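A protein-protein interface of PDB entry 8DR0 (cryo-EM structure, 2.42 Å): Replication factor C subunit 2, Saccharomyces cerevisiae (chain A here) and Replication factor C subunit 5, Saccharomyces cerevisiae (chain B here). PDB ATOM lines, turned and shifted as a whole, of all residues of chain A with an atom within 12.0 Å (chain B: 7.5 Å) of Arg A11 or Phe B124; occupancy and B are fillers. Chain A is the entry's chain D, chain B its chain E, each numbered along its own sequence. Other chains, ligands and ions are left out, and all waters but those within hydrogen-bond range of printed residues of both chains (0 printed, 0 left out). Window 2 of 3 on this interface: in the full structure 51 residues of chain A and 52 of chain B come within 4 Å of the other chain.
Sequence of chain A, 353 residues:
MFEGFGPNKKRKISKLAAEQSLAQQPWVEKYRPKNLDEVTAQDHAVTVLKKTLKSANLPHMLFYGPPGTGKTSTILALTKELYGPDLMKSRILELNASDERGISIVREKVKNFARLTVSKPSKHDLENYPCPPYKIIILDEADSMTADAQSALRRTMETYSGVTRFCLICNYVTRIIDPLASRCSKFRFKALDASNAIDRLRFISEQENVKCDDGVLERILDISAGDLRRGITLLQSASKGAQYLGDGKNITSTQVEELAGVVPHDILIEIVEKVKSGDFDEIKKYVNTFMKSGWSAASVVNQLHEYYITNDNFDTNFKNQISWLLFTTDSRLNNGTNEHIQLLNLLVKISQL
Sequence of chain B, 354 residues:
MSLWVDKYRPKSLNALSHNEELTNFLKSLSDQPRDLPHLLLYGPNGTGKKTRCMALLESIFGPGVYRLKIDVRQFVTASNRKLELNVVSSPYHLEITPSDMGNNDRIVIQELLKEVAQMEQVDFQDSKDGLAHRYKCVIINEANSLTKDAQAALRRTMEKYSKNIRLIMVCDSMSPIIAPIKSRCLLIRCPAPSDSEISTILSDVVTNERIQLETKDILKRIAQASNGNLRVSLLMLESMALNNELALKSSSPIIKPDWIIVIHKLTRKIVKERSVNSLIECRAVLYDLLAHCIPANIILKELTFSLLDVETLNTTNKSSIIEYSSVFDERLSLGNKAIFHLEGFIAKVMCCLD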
ATOM      1  N   LYS A  10      12.193 -12.999 -26.747  1.00  0.00           N
ATOM      2  CA  LYS A  10      12.098 -11.601 -27.153  1.00  0.00           C
ATOM      3  C   LYS A  10      10.645 -11.199 -27.374  1.00  0.00           C
ATOM      4  O   LYS A  10       9.895 -11.892 -28.061  1.00  0.00           O
ATOM      5  CB  LYS A  10      12.911 -11.358 -28.425  1.00  0.00           C
ATOM      6  N   ARG A  11      10.251 -10.068 -26.784  1.00  0.00           N
ATOM      7  CA  ARG A  11       8.882  -9.590 -26.939  1.00  0.00           C
ATOM      8  C   ARG A  11       8.568  -9.249 -28.390  1.00  0.00           C
ATOM      9  O   ARG A  11       7.452  -9.505 -28.856  1.00  0.00           O
ATOM     10  CB  ARG A  11       8.646  -8.372 -26.047  1.00  0.00           C
ATOM     11  N   LYS A  12       9.526  -8.664 -29.109  1.00  0.00           N
ATOM     12  CA  LYS A  12       9.338  -8.290 -30.507  1.00  0.00           C
ATOM     13  C   LYS A  12       8.435  -7.068 -30.617  1.00  0.00           C
ATOM     14  O   LYS A  12       7.643  -6.788 -29.711  1.00  0.00           O
ATOM     15  CB  LYS A  12       8.755  -9.458 -31.307  1.00  0.00           C
ATOM     16  CG  LYS A  12       9.166  -9.473 -32.771  1.00  0.00           C
ATOM     17  CD  LYS A  12      10.603  -9.938 -32.943  1.00  0.00           C
ATOM     18  CE  LYS A  12      10.947 -10.145 -34.409  1.00  0.00           C
ATOM     19  NZ  LYS A  12      12.231 -10.880 -34.582  1.00  0.00           N
ATOM     20  N   ILE A  13       8.549  -6.335 -31.722  1.00  0.00           N
ATOM     21  CA  ILE A  13       7.776  -5.122 -31.954  1.00  0.00           C
ATOM     22  C   ILE A  13       7.122  -5.219 -33.324  1.00  0.00           C
ATOM     23  O   ILE A  13       7.757  -5.632 -34.300  1.00  0.00           O
ATOM     24  CB  ILE A  13       8.650  -3.851 -31.867  1.00  0.00           C
ATOM     25  CG1 ILE A  13       9.672  -3.964 -30.730  1.00  0.00           C
ATOM     26  CG2 ILE A  13       7.769  -2.627 -31.669  1.00  0.00           C
ATOM     27  CD1 ILE A  13      10.694  -2.843 -30.709  1.00  0.00           C
ATOM     28  N   SER A  14       5.849  -4.838 -33.394  1.00  0.00           N
ATOM     29  CA  SER A  14       5.136  -4.837 -34.661  1.00  0.00           C
ATOM     30  C   SER A  14       5.741  -3.811 -35.612  1.00  0.00           C
ATOM     31  O   SER A  14       6.273  -2.779 -35.194  1.00  0.00           O
ATOM     32  CB  SER A  14       3.655  -4.536 -34.441  1.00  0.00           C
ATOM     33  OG  SER A  14       3.482  -3.292 -33.783  1.00  0.00           O
ATOM     34  N   LYS A  15       5.655  -4.104 -36.907  1.00  0.00           N
ATOM     35  CA  LYS A  15       6.190  -3.195 -37.910  1.00  0.00           C
ATOM     36  C   LYS A  15       5.485  -1.847 -37.828  1.00  0.00           C
ATOM     37  O   LYS A  15       4.277  -1.770 -37.590  1.00  0.00           O
ATOM     38  CB  LYS A  15       6.031  -3.795 -39.307  1.00  0.00           C
ATOM     39  CG  LYS A  15       6.911  -5.011 -39.556  1.00  0.00           C
ATOM     40  CD  LYS A  15       6.888  -5.431 -41.017  1.00  0.00           C
ATOM     41  CE  LYS A  15       7.864  -6.567 -41.279  1.00  0.00           C
ATOM     42  NZ  LYS A  15       8.003  -6.864 -42.732  1.00  0.00           N
ATOM     43  N   LEU A  16       6.251  -0.780 -38.031  1.00  0.00           N
ATOM     44  CA  LEU A  16       5.760   0.582 -37.885  1.00  0.00           C
ATOM     45  C   LEU A  16       5.488   1.187 -39.256  1.00  0.00           C
ATOM     46  O   LEU A  16       6.309   1.073 -40.172  1.00  0.00           O
ATOM     47  CB  LEU A  16       6.770   1.435 -37.113  1.00  0.00           C
ATOM     48  CG  LEU A  16       6.263   2.736 -36.485  1.00  0.00           C
ATOM     49  CD1 LEU A  16       7.232   3.220 -35.421  1.00  0.00           C
ATOM     50  CD2 LEU A  16       6.055   3.811 -37.536  1.00  0.00           C
ATOM     51  N   GLN B 121      15.882  -2.857 -35.617  1.00  0.00           N
ATOM     52  CA  GLN B 121      15.785  -3.323 -34.241  1.00  0.00           C
ATOM     53  C   GLN B 121      14.470  -4.064 -34.030  1.00  0.00           C
ATOM     54  O   GLN B 121      13.405  -3.587 -34.431  1.00  0.00           O
ATOM     55  CB  GLN B 121      15.891  -2.145 -33.275  1.00  0.00           C
ATOM     56  CG  GLN B 121      15.766  -2.531 -31.810  1.00  0.00           C
ATOM     57  CD  GLN B 121      16.233  -1.436 -30.865  1.00  0.00           C
ATOM     58  OE1 GLN B 121      16.662  -1.715 -29.744  1.00  0.00           O
ATOM     59  NE2 GLN B 121      16.147  -0.185 -31.307  1.00  0.00           N
ATOM     60  N   VAL B 122      14.549  -5.235 -33.397  1.00  0.00           N
ATOM     61  CA  VAL B 122      13.371  -6.056 -33.139  1.00  0.00           C
ATOM     62  C   VAL B 122      13.319  -6.430 -31.664  1.00  0.00           C
ATOM     63  O   VAL B 122      12.694  -7.427 -31.287  1.00  0.00           O
ATOM     64  CB  VAL B 122      13.368  -7.315 -34.026  1.00  0.00           C
ATOM     65  CG1 VAL B 122      13.265  -6.930 -35.494  1.00  0.00           C
ATOM     66  CG2 VAL B 122      14.616  -8.153 -33.774  1.00  0.00           C
ATOM     67  N   ASP B 123      13.973  -5.635 -30.820  1.00  0.00           N
ATOM     68  CA  ASP B 123      13.996  -5.866 -29.382  1.00  0.00           C
ATOM     69  C   ASP B 123      13.058  -4.882 -28.695  1.00  0.00           C
ATOM     70  O   ASP B 123      13.187  -3.666 -28.872  1.00  0.00           O
ATOM     71  CB  ASP B 123      15.415  -5.716 -28.830  1.00  0.00           C
ATOM     72  CG  ASP B 123      16.381  -6.719 -29.428  1.00  0.00           C
ATOM     73  OD1 ASP B 123      16.021  -7.367 -30.432  1.00  0.00           O
ATOM     74  OD2 ASP B 123      17.501  -6.860 -28.894  1.00  0.00           O
ATOM     75  N   PHE B 124      12.121  -5.412 -27.908  1.00  0.00           N
ATOM     76  CA  PHE B 124      11.119  -4.594 -27.226  1.00  0.00           C
ATOM     77  C   PHE B 124      11.776  -3.912 -26.029  1.00  0.00           C
ATOM     78  O   PHE B 124      11.703  -4.370 -24.886  1.00  0.00           O
ATOM     79  CB  PHE B 124       9.928  -5.445 -26.804  1.00  0.00           C
ATOM     80  CG  PHE B 124       8.814  -4.657 -26.175  1.00  0.00           C
ATOM     81  CD1 PHE B 124       8.010  -3.833 -26.945  1.00  0.00           C
ATOM     82  CD2 PHE B 124       8.569  -4.742 -24.814  1.00  0.00           C
ATOM     83  CE1 PHE B 124       6.984  -3.108 -26.369  1.00  0.00           C
ATOM     84  CE2 PHE B 124       7.545  -4.019 -24.234  1.00  0.00           C
ATOM     85  CZ  PHE B 124       6.752  -3.200 -25.012  1.00  0.00           C
ATOM     86  N   GLN B 125      12.434  -2.788 -26.310  1.00  0.00           N
ATOM     87  CA  GLN B 125      13.095  -1.986 -25.281  1.00  0.00           C
ATOM     88  C   GLN B 125      12.174  -0.819 -24.930  1.00  0.00           C
ATOM     89  O   GLN B 125      12.303   0.293 -25.441  1.00  0.00           O
ATOM     90  CB  GLN B 125      14.460  -1.509 -25.767  1.00  0.00           C
ATOM     91  CG  GLN B 125      15.393  -2.632 -26.189  1.00  0.00           C
ATOM     92  CD  GLN B 125      16.684  -2.120 -26.796  1.00  0.00           C
ATOM     93  OE1 GLN B 125      16.813  -0.933 -27.098  1.00  0.00           O
ATOM     94  NE2 GLN B 125      17.648  -3.014 -26.978  1.00  0.00           N
ATOM     95  N   ASP B 126      11.229  -1.091 -24.033  1.00  0.00           N
ATOM     96  CA  ASP B 126      10.250  -0.085 -23.644  1.00  0.00           C
ATOM     97  C   ASP B 126      10.947   1.157 -23.102  1.00  0.00           C
ATOM     98  O   ASP B 126      11.866   1.062 -22.284  1.00  0.00           O
ATOM     99  CB  ASP B 126       9.296  -0.656 -22.596  1.00  0.00           C
ATOM    100  CG  ASP B 126       8.140   0.275 -22.289  1.00  0.00           C
ATOM    101  OD1 ASP B 126       8.011   1.313 -22.972  1.00  0.00           O
ATOM    102  OD2 ASP B 126       7.358  -0.030 -21.364  1.00  0.00           O
ATOM    103  N   SER B 127      10.506   2.322 -23.565  1.00  0.00           N
ATOM    104  CA  SER B 127      11.074   3.605 -23.180  1.00  0.00           C
ATOM    105  C   SER B 127      10.136   4.318 -22.209  1.00  0.00           C
ATOM    106  O   SER B 127       9.101   3.788 -21.797  1.00  0.00           O
ATOM    107  CB  SER B 127      11.338   4.464 -24.418  1.00  0.00           C
ATOM    108  OG  SER B 127      10.143   5.059 -24.890  1.00  0.00           O
ATOM    109  N   GLY B 130       6.575   4.873 -23.304  1.00  0.00           N
ATOM    110  CA  GLY B 130       5.776   3.673 -23.379  1.00  0.00           C
ATOM    111  C   GLY B 130       5.987   2.858 -24.638  1.00  0.00           C
ATOM    112  O   GLY B 130       5.594   1.686 -24.672  1.00  0.00           O
ATOM    113  N   LEU B 131       6.592   3.442 -25.667  1.00  0.00           N
ATOM    114  CA  LEU B 131       6.885   2.744 -26.908  1.00  0.00           C
ATOM    115  C   LEU B 131       8.340   2.297 -26.924  1.00  0.00           C
ATOM    116  O   LEU B 131       9.223   2.970 -26.387  1.00  0.00           O
ATOM    117  CB  LEU B 131       6.598   3.637 -28.118  1.00  0.00           C
ATOM    118  CG  LEU B 131       5.191   4.235 -28.184  1.00  0.00           C
ATOM    119  CD1 LEU B 131       5.039   5.107 -29.420  1.00  0.00           C
ATOM    120  CD2 LEU B 131       4.133   3.142 -28.164  1.00  0.00           C
ATOM    121  N   ALA B 132       8.580   1.148 -27.548  1.00  0.00           N
ATOM    122  CA  ALA B 132       9.919   0.577 -27.578  1.00  0.00           C
ATOM    123  C   ALA B 132      10.867   1.458 -28.383  1.00  0.00           C
ATOM    124  O   ALA B 132      10.470   2.137 -29.332  1.00  0.00           O
ATOM    125  CB  ALA B 132       9.882  -0.830 -28.173  1.00  0.00           C
ATOM    126  N   HIS B 133      12.138   1.439 -27.988  1.00  0.00           N
ATOM    127  CA  HIS B 133      13.153   2.195 -28.710  1.00  0.00           C
ATOM    128  C   HIS B 133      13.277   1.675 -30.136  1.00  0.00           C
ATOM    129  O   HIS B 133      13.149   0.475 -30.392  1.00  0.00           O
ATOM    130  CB  HIS B 133      14.498   2.097 -27.991  1.00  0.00           C
ATOM    131  CG  HIS B 133      14.582   2.938 -26.756  1.00  0.00           C
ATOM    132  ND1 HIS B 133      14.697   2.399 -25.493  1.00  0.00           N
ATOM    133  CD2 HIS B 133      14.568   4.283 -26.591  1.00  0.00           C
ATOM    134  CE1 HIS B 133      14.750   3.374 -24.603  1.00  0.00           C
ATOM    135  NE2 HIS B 133      14.674   4.527 -25.244  1.00  0.00           N
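Of the 7 printed residues of chain A, 3 touch a printed residue of chain B.
Printed residues of chain A that touch a printed residue of chain B: Arg A11, Lys A12 and Ile A13.
Hydrophobic or aromatic side chains of chain A that line the printed part of chain B: Ile A13.
Among the printed residues, pairs that only touch across the chains: Arg A11 with Phe B124 (3.3 Å), Lys A12 with Val B122 (3.6 Å), Lys A12 with Phe B124 (3.9 Å), Ile A13 with Asp B123 (3.2 Å), Ile A13 with Phe B124 (3.8 Å) and Ile A13 with Ala B132 (3.3 Å).
Arg A11 touches just one residue of chain B: Phe B124.
Printed residues of chain B within 4 Å of Lys A12: Val B122 and Phe B124.
Of the printed residues of chain B, Ile A13 touches Asp B123 (3.2 Å), Phe B124 (3.8 Å) and Ala B132 (3.3 Å).
Ser A14 touches none of the printed residues of chain B.
Val B122 touches just one residue of chain A: Lys A12 (3.6 Å).
Of chain A, only Ile A13 comes within 4 Å of Asp B123.
Of chain A, only Arg A11, Lys A12 and Ile A13 come within 4 Å of Phe B124.
No residue of chain A comes within 4 Å of Gln B125.
Of chain A, only Ile A13 comes within 4 Å of Ala B132.
The nearest printed residue of chain B that does not touch Lys A12 is Asp B123 (5.2 Å).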
